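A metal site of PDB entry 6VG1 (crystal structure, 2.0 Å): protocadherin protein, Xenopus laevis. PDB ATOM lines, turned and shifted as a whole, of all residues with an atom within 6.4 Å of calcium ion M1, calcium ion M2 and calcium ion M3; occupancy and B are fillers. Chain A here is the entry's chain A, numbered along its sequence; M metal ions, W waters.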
ATOM      1  N   GLU A   9       4.032  14.460  10.330  1.00  0.00           N
ATOM      2  CA  GLU A   9       3.725  14.306  11.744  1.00  0.00           C
ATOM      3  C   GLU A   9       2.269  13.891  11.949  1.00  0.00           C
ATOM      4  O   GLU A   9       1.421  14.102  11.081  1.00  0.00           O
ATOM      5  CB  GLU A   9       4.014  15.608  12.509  1.00  0.00           C
ATOM      6  CG  GLU A   9       3.080  16.755  12.201  1.00  0.00           C
ATOM      7  CD  GLU A   9       3.170  17.884  13.220  1.00  0.00           C
ATOM      8  OE1 GLU A   9       3.285  17.583  14.435  1.00  0.00           O
ATOM      9  OE2 GLU A   9       3.137  19.074  12.825  1.00  0.00           O
ATOM     10  N   GLU A  10       1.985  13.279  13.099  1.00  0.00           N
ATOM     11  CA  GLU A  10       0.637  12.871  13.472  1.00  0.00           C
ATOM     12  C   GLU A  10      -0.011  12.001  12.388  1.00  0.00           C
ATOM     13  O   GLU A  10      -1.209  12.105  12.124  1.00  0.00           O
ATOM     14  CB  GLU A  10      -0.256  14.082  13.768  1.00  0.00           C
ATOM     15  CG  GLU A  10       0.395  15.251  14.472  1.00  0.00           C
ATOM     16  CD  GLU A  10       0.062  15.322  15.963  1.00  0.00           C
ATOM     17  OE1 GLU A  10      -0.365  14.306  16.538  1.00  0.00           O
ATOM     18  OE2 GLU A  10       0.248  16.415  16.543  1.00  0.00           O
ATOM     19  N   ARG A  57       2.414   7.714  18.166  1.00  0.00           N
ATOM     20  CA  ARG A  57       2.077   9.053  17.700  1.00  0.00           C
ATOM     21  C   ARG A  57       3.330   9.896  17.549  1.00  0.00           C
ATOM     22  O   ARG A  57       4.216   9.875  18.414  1.00  0.00           O
ATOM     23  CB  ARG A  57       1.111   9.684  18.689  1.00  0.00           C
ATOM     24  CG  ARG A  57       0.639  11.077  18.351  1.00  0.00           C
ATOM     25  CD  ARG A  57      -0.322  11.545  19.443  1.00  0.00           C
ATOM     26  NE  ARG A  57      -0.832  12.894  19.229  1.00  0.00           N
ATOM     27  CZ  ARG A  57      -0.235  13.985  19.680  1.00  0.00           C
ATOM     28  NH1 ARG A  57       0.892  13.910  20.366  1.00  0.00           N
ATOM     29  NH2 ARG A  57      -0.778  15.176  19.453  1.00  0.00           N
ATOM     30  N   ILE A  58       3.409  10.638  16.451  1.00  0.00           N
ATOM     31  CA  ILE A  58       4.555  11.494  16.158  1.00  0.00           C
ATOM     32  C   ILE A  58       4.073  12.942  16.101  1.00  0.00           C
ATOM     33  O   ILE A  58       3.453  13.343  15.112  1.00  0.00           O
ATOM     34  CB  ILE A  58       5.254  11.112  14.851  1.00  0.00           C
ATOM     35  CG1 ILE A  58       5.802   9.692  14.921  1.00  0.00           C
ATOM     36  CG2 ILE A  58       6.366  12.110  14.538  1.00  0.00           C
ATOM     37  CD1 ILE A  58       6.334   9.180  13.591  1.00  0.00           C
ATOM     38  N   ASP A  59       4.368  13.717  17.150  1.00  0.00           N
ATOM     39  CA  ASP A  59       3.982  15.127  17.223  1.00  0.00           C
ATOM     40  C   ASP A  59       5.228  15.990  17.108  1.00  0.00           C
ATOM     41  O   ASP A  59       6.019  16.078  18.052  1.00  0.00           O
ATOM     42  CB  ASP A  59       3.239  15.407  18.529  1.00  0.00           C
ATOM     43  CG  ASP A  59       2.666  16.821  18.586  1.00  0.00           C
ATOM     44  OD1 ASP A  59       2.821  17.577  17.601  1.00  0.00           O
ATOM     45  OD2 ASP A  59       2.051  17.174  19.614  1.00  0.00           O
ATOM     46  N   ARG A  60       5.380  16.659  15.962  1.00  0.00           N
ATOM     47  CA  ARG A  60       6.576  17.477  15.745  1.00  0.00           C
ATOM     48  C   ARG A  60       6.706  18.553  16.819  1.00  0.00           C
ATOM     49  O   ARG A  60       7.786  18.767  17.370  1.00  0.00           O
ATOM     50  CB  ARG A  60       6.539  18.112  14.360  1.00  0.00           C
ATOM     51  CG  ARG A  60       7.914  18.539  13.852  1.00  0.00           C
ATOM     52  CD  ARG A  60       7.847  19.729  12.925  1.00  0.00           C
ATOM     53  NE  ARG A  60       7.120  20.842  13.545  1.00  0.00           N
ATOM     54  CZ  ARG A  60       7.562  21.545  14.585  1.00  0.00           C
ATOM     55  NH1 ARG A  60       8.733  21.247  15.128  1.00  0.00           N
ATOM     56  NH2 ARG A  60       6.837  22.536  15.067  1.00  0.00           N
ATOM     57  N   GLU A  61       5.612  19.248  17.120  1.00  0.00           N
ATOM     58  CA  GLU A  61       5.654  20.336  18.087  1.00  0.00           C
ATOM     59  C   GLU A  61       6.062  19.866  19.486  1.00  0.00           C
ATOM     60  O   GLU A  61       6.413  20.710  20.320  1.00  0.00           O
ATOM     61  CB  GLU A  61       4.296  21.036  18.139  1.00  0.00           C
ATOM     62  CG  GLU A  61       4.015  21.990  16.961  1.00  0.00           C
ATOM     63  CD  GLU A  61       3.485  21.299  15.723  1.00  0.00           C
ATOM     64  OE1 GLU A  61       2.551  20.476  15.828  1.00  0.00           O
ATOM     65  OE2 GLU A  61       4.000  21.588  14.626  1.00  0.00           O
ATOM     66  N   ARG A  62       6.048  18.558  19.754  1.00  0.00           N
ATOM     67  CA  ARG A  62       6.443  18.030  21.051  1.00  0.00           C
ATOM     68  C   ARG A  62       7.886  17.556  21.088  1.00  0.00           C
ATOM     69  O   ARG A  62       8.493  17.545  22.162  1.00  0.00           O
ATOM     70  CB  ARG A  62       5.531  16.874  21.463  1.00  0.00           C
ATOM     71  CG  ARG A  62       5.945  16.200  22.761  1.00  0.00           C
ATOM     72  CD  ARG A  62       4.949  15.116  23.181  1.00  0.00           C
ATOM     73  NE  ARG A  62       4.843  14.055  22.179  1.00  0.00           N
ATOM     74  CZ  ARG A  62       5.682  13.033  22.072  1.00  0.00           C
ATOM     75  NH1 ARG A  62       6.716  12.932  22.894  1.00  0.00           N
ATOM     76  NH2 ARG A  62       5.499  12.120  21.131  1.00  0.00           N
ATOM     77  N   ASP A  95       6.213  19.232   8.838  1.00  0.00           N
ATOM     78  CA  ASP A  95       5.317  19.946   9.736  1.00  0.00           C
ATOM     79  C   ASP A  95       3.920  20.034   9.124  1.00  0.00           C
ATOM     80  O   ASP A  95       3.767  20.272   7.925  1.00  0.00           O
ATOM     81  CB  ASP A  95       5.846  21.347  10.030  1.00  0.00           C
ATOM     82  CG  ASP A  95       4.900  22.167  10.895  1.00  0.00           C
ATOM     83  OD1 ASP A  95       3.897  21.620  11.405  1.00  0.00           O
ATOM     84  OD2 ASP A  95       5.155  23.380  11.071  1.00  0.00           O
ATOM     85  N   ILE A  96       2.906  19.854   9.983  1.00  0.00           N
ATOM     86  CA  ILE A  96       1.508  20.021   9.612  1.00  0.00           C
ATOM     87  C   ILE A  96       0.973  21.221  10.367  1.00  0.00           C
ATOM     88  O   ILE A  96       1.470  21.569  11.445  1.00  0.00           O
ATOM     89  CB  ILE A  96       0.700  18.747   9.900  1.00  0.00           C
ATOM     90  CG1 ILE A  96      -0.536  18.683   9.003  1.00  0.00           C
ATOM     91  CG2 ILE A  96       0.271  18.685  11.354  1.00  0.00           C
ATOM     92  CD1 ILE A  96      -0.212  18.507   7.525  1.00  0.00           C
ATOM     93  N   ASN A  97      -0.052  21.855   9.796  1.00  0.00           N
ATOM     94  CA  ASN A  97      -0.593  23.105  10.334  1.00  0.00           C
ATOM     95  C   ASN A  97      -1.716  22.840  11.342  1.00  0.00           C
ATOM     96  O   ASN A  97      -2.820  23.372  11.243  1.00  0.00           O
ATOM     97  CB  ASN A  97      -1.085  23.961   9.177  1.00  0.00           C
ATOM     98  CG  ASN A  97      -1.379  25.392   9.599  1.00  0.00           C
ATOM     99  OD1 ASN A  97      -0.772  25.909  10.543  1.00  0.00           O
ATOM    100  ND2 ASN A  97      -2.313  26.030   8.909  1.00  0.00           N
ATOM    101  N   ASP A  98      -1.409  22.006  12.331  1.00  0.00           N
ATOM    102  CA  ASP A  98      -2.370  21.628  13.360  1.00  0.00           C
ATOM    103  C   ASP A  98      -2.324  22.548  14.565  1.00  0.00           C
ATOM    104  O   ASP A  98      -2.829  22.185  15.626  1.00  0.00           O
ATOM    105  CB  ASP A  98      -2.129  20.177  13.803  1.00  0.00           C
ATOM    106  CG  ASP A  98      -0.666  19.894  14.150  1.00  0.00           C
ATOM    107  OD1 ASP A  98       0.192  20.793  13.990  1.00  0.00           O
ATOM    108  OD2 ASP A  98      -0.384  18.752  14.569  1.00  0.00           O
ATOM    109  N   ASN A  99      -1.746  23.737  14.418  1.00  0.00           N
ATOM    110  CA  ASN A  99      -1.745  24.721  15.488  1.00  0.00           C
ATOM    111  C   ASN A  99      -2.028  26.086  14.903  1.00  0.00           C
ATOM    112  O   ASN A  99      -1.458  26.465  13.864  1.00  0.00           O
ATOM    113  CB  ASN A  99      -0.419  24.737  16.246  1.00  0.00           C
ATOM    114  CG  ASN A  99      -0.312  23.609  17.249  1.00  0.00           C
ATOM    115  OD1 ASN A  99      -1.112  23.526  18.189  1.00  0.00           O
ATOM    116  ND2 ASN A  99       0.649  22.724  17.062  1.00  0.00           N
ATOM    117  N   SER A 100      -2.898  26.836  15.596  1.00  0.00           N
ATOM    118  CA  SER A 100      -3.346  28.134  15.174  1.00  0.00           C
ATOM    119  C   SER A 100      -2.736  29.213  16.045  1.00  0.00           C
ATOM    120  O   SER A 100      -2.428  28.977  17.216  1.00  0.00           O
ATOM    121  CB  SER A 100      -4.860  28.190  15.270  1.00  0.00           C
ATOM    122  OG  SER A 100      -5.294  27.592  16.492  1.00  0.00           O
ATOM    123  N   PRO A 101      -2.592  30.420  15.517  1.00  0.00           N
ATOM    124  CA  PRO A 101      -2.071  31.525  16.347  1.00  0.00           C
ATOM    125  C   PRO A 101      -2.921  31.724  17.586  1.00  0.00           C
ATOM    126  O   PRO A 101      -4.148  31.641  17.541  1.00  0.00           O
ATOM    127  CB  PRO A 101      -2.124  32.733  15.411  1.00  0.00           C
ATOM    128  CG  PRO A 101      -2.072  32.152  14.023  1.00  0.00           C
ATOM    129  CD  PRO A 101      -2.826  30.829  14.116  1.00  0.00           C
ATOM    130  N   ASP A 129       2.312  30.765  17.385  1.00  0.00           N
ATOM    131  CA  ASP A 129       1.854  29.635  16.580  1.00  0.00           C
ATOM    132  C   ASP A 129       2.916  28.560  16.701  1.00  0.00           C
ATOM    133  O   ASP A 129       4.063  28.778  16.290  1.00  0.00           O
ATOM    134  CB  ASP A 129       1.648  30.040  15.122  1.00  0.00           C
ATOM    135  CG  ASP A 129       1.006  28.936  14.283  1.00  0.00           C
ATOM    136  OD1 ASP A 129       0.893  27.762  14.719  1.00  0.00           O
ATOM    137  OD2 ASP A 129       0.632  29.258  13.131  1.00  0.00           O
ATOM    138  N   GLU A 130       2.555  27.414  17.281  1.00  0.00           N
ATOM    139  CA  GLU A 130       3.545  26.395  17.601  1.00  0.00           C
ATOM    140  C   GLU A 130       4.040  25.627  16.375  1.00  0.00           C
ATOM    141  O   GLU A 130       4.915  24.773  16.541  1.00  0.00           O
ATOM    142  CB  GLU A 130       2.964  25.422  18.636  1.00  0.00           C
ATOM    143  CG  GLU A 130       2.762  26.058  20.001  1.00  0.00           C
ATOM    144  CD  GLU A 130       2.448  25.039  21.081  1.00  0.00           C
ATOM    145  OE1 GLU A 130       2.215  23.860  20.732  1.00  0.00           O
ATOM    146  OE2 GLU A 130       2.432  25.417  22.270  1.00  0.00           O
ATOM    147  N   ASP A 131       3.510  25.891  15.189  1.00  0.00           N
ATOM    148  CA  ASP A 131       4.087  25.339  13.967  1.00  0.00           C
ATOM    149  C   ASP A 131       5.343  26.122  13.598  1.00  0.00           C
ATOM    150  O   ASP A 131       5.775  27.024  14.335  1.00  0.00           O
ATOM    151  CB  ASP A 131       3.046  25.370  12.854  1.00  0.00           C
ATOM    152  CG  ASP A 131       1.743  24.686  13.250  1.00  0.00           C
ATOM    153  OD1 ASP A 131       1.779  23.622  13.926  1.00  0.00           O
ATOM    154  OD2 ASP A 131       0.661  25.220  12.888  1.00  0.00           O
ATOM    155  N   VAL A 132       5.956  25.782  12.460  1.00  0.00           N
ATOM    156  CA  VAL A 132       7.151  26.480  12.003  1.00  0.00           C
ATOM    157  C   VAL A 132       6.973  26.876  10.538  1.00  0.00           C
ATOM    158  O   VAL A 132       6.019  26.471   9.876  1.00  0.00           O
ATOM    159  CB  VAL A 132       8.436  25.619  12.174  1.00  0.00           C
ATOM    160  CG1 VAL A 132       8.700  25.320  13.641  1.00  0.00           C
ATOM    161  CG2 VAL A 132       8.317  24.336  11.371  1.00  0.00           C
ATOM    162  N   VAL A 134       6.130  28.503   7.067  1.00  0.00           N
ATOM    163  CA  VAL A 134       4.921  29.197   6.634  1.00  0.00           C
ATOM    164  C   VAL A 134       3.789  28.959   7.618  1.00  0.00           C
ATOM    165  O   VAL A 134       2.915  29.814   7.804  1.00  0.00           O
ATOM    166  CB  VAL A 134       4.518  28.771   5.214  1.00  0.00           C
ATOM    167  CG1 VAL A 134       5.662  29.002   4.248  1.00  0.00           C
ATOM    168  CG2 VAL A 134       4.053  27.314   5.209  1.00  0.00           C
ATOM    169  N   ASN A 135       3.772  27.789   8.264  1.00  0.00           N
ATOM    170  CA  ASN A 135       2.738  27.485   9.248  1.00  0.00           C
ATOM    171  C   ASN A 135       2.867  28.315  10.514  1.00  0.00           C
ATOM    172  O   ASN A 135       2.019  28.190  11.404  1.00  0.00           O
ATOM    173  CB  ASN A 135       2.762  26.005   9.591  1.00  0.00           C
ATOM    174  CG  ASN A 135       2.343  25.139   8.424  1.00  0.00           C
ATOM    175  OD1 ASN A 135       1.883  25.657   7.407  1.00  0.00           O
ATOM    176  ND2 ASN A 135       2.493  23.830   8.569  1.00  0.00           N
ATOM    177  N   SER A 136       3.888  29.159  10.603  1.00  0.00           N
ATOM    178  CA  SER A 136       4.053  30.079  11.724  1.00  0.00           C
ATOM    179  C   SER A 136       3.324  31.388  11.419  1.00  0.00           C
ATOM    180  O   SER A 136       2.797  31.598  10.315  1.00  0.00           O
ATOM    181  CB  SER A 136       5.522  30.337  11.994  1.00  0.00           C
ATOM    182  OG  SER A 136       6.081  31.166  10.978  1.00  0.00           O
ATOM    183  N   ILE A 137       3.307  32.294  12.385  1.00  0.00           N
ATOM    184  CA  ILE A 137       2.614  33.573  12.222  1.00  0.00           C
ATOM    185  C   ILE A 137       3.328  34.386  11.153  1.00  0.00           C
ATOM    186  O   ILE A 137       4.519  34.696  11.278  1.00  0.00           O
ATOM    187  CB  ILE A 137       2.562  34.332  13.550  1.00  0.00           C
ATOM    188  CG1 ILE A 137       1.671  33.571  14.537  1.00  0.00           C
ATOM    189  CG2 ILE A 137       2.033  35.751  13.341  1.00  0.00           C
ATOM    190  CD1 ILE A 137       1.676  34.139  15.954  1.00  0.00           C
ATOM    191  N   ASP A 186      -1.321  32.735   9.814  1.00  0.00           N
ATOM    192  CA  ASP A 186      -0.172  32.028   9.273  1.00  0.00           C
ATOM    193  C   ASP A 186      -0.340  31.784   7.771  1.00  0.00           C
ATOM    194  O   ASP A 186      -1.362  32.122   7.166  1.00  0.00           O
ATOM    195  CB  ASP A 186       0.035  30.702  10.024  1.00  0.00           C
ATOM    196  CG  ASP A 186      -1.174  29.755   9.920  1.00  0.00           C
ATOM    197  OD1 ASP A 186      -1.920  29.819   8.913  1.00  0.00           O
ATOM    198  OD2 ASP A 186      -1.370  28.946  10.852  1.00  0.00           O
ATOM    199  N   GLY A 187       0.678  31.151   7.175  1.00  0.00           N
ATOM    200  CA  GLY A 187       0.709  30.935   5.744  1.00  0.00           C
ATOM    201  C   GLY A 187       0.049  29.630   5.317  1.00  0.00           C
ATOM    202  O   GLY A 187      -0.428  28.837   6.138  1.00  0.00           O
ATOM    203  N   ARG A 192      -4.983  29.701   9.441  1.00  0.00           N
ATOM    204  CA  ARG A 192      -5.563  29.728  10.774  1.00  0.00           C
ATOM    205  C   ARG A 192      -5.268  31.074  11.422  1.00  0.00           C
ATOM    206  O   ARG A 192      -4.110  31.512  11.463  1.00  0.00           O
ATOM    207  CB  ARG A 192      -5.038  28.577  11.622  1.00  0.00           C
ATOM    208  CG  ARG A 192      -5.513  27.217  11.099  1.00  0.00           C
ATOM    209  CD  ARG A 192      -4.660  26.056  11.584  1.00  0.00           C
ATOM    210  NE  ARG A 192      -4.939  25.651  12.957  1.00  0.00           N
ATOM    211  CZ  ARG A 192      -5.612  24.558  13.294  1.00  0.00           C
ATOM    212  NH1 ARG A 192      -6.084  23.747  12.365  1.00  0.00           N
ATOM    213  NH2 ARG A 192      -5.800  24.271  14.579  1.00  0.00           N
HETATM  214 CA    CA M   1       2.381  21.355  13.231  1.00  0.00          CA
HETATM  215 CA    CA M   2       1.469  18.408  15.794  1.00  0.00          CA
HETATM  216 CA    CA M   3       0.015  27.340  12.241  1.00  0.00          CA
HETATM  217  O   HOH W   1       0.017  18.884  18.302  1.00  0.00           O
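Six residues have an atom within 4 Å of calcium ion M1: Glu 9, Glu 61, Asp 95, Ile 96, Asp 98 and Asp 131.
The side-chain carboxylate (OD2) of Asp 129 binds calcium ion M3 (2.2 Å).
OD2 of Asp 131 is bound to calcium ion M3 (2.3 Å).
Calcium ion M3 is bound by O of Asn 135.
Calcium ion M3 is bound by OD1 of Asn 97, at 2.4 Å.
Calcium ion M3 is bound by the backbone carbonyl oxygen (O) of Asn 99 (2.4 Å).
The side-chain carboxylate (OD2) of Asp 186 binds calcium ion M3, 2.5 Å away.
Calcium ion M3 is bound by OD1 of Asp 129.
Calcium ion M3 has seven donor atoms within binding distance.
The side-chain amide nitrogen (ND2) of Asn 99 lies close to the side-chain carboxylate (OE1) of Glu 61, at 3.2 Å.
The side-chain carboxylate (OE2) of Glu 61 lies close to the guanidinium group (NH2) of Arg 60.
The guanidinium group (NH1) of Arg 192 lies close to the backbone carbonyl oxygen (O) of Asn 97, 3.5 Å away.
The side-chain carboxylate (OD1) of Asp 95 sits close to the guanidinium group (NE) of Arg 60 (3.9 Å).
OD2 of Asp 59 lies within salt-bridge range of NH2 of Arg 57 (3.5 Å).
The side-chain carboxylate of Glu 10 lies within salt-bridge range of the guanidinium group of Arg 57, 3.1 Å away.
The backbone NH (N) of Glu 10 is in hydrogen-bond range of the backbone carbonyl oxygen (O) of Ile 58.
OD1 of Asp 186 is in hydrogen-bond range of N of Arg 192 (3.1 Å).
Calcium ion M1 is bound by O of Ile 96, OE2 of Glu 61, OD1 of Asp 98, OD1 of Asp 95, OE2 of Glu 9, OD1 of Asp 131 and OE1 of Glu 61.
Of the 26 residues printed, 6 come within 4 Å of calcium ion M3.
The nearest printed residue that does not touch calcium ion M2 is Arg 60 (4.3 Å).
OD2 of Asp 98 is bound to calcium ion M2 (2.2 Å).
The side-chain carboxylate (OE1) of Glu 61 is bound to calcium ion M2, at 2.3 Å.
Calcium ion M2 is bound by OD1 of Asp 59, at 2.4 Å.
The side-chain carboxylate (OE1) of Glu 9 is bound to calcium ion M2 (2.4 Å).
OE2 of Glu 10 binds calcium ion M2 (2.5 Å).
Calcium ion M2 has five donor atoms within binding distance.
Slightly farther from calcium ion M2 lies water W1 (2.9 Å).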
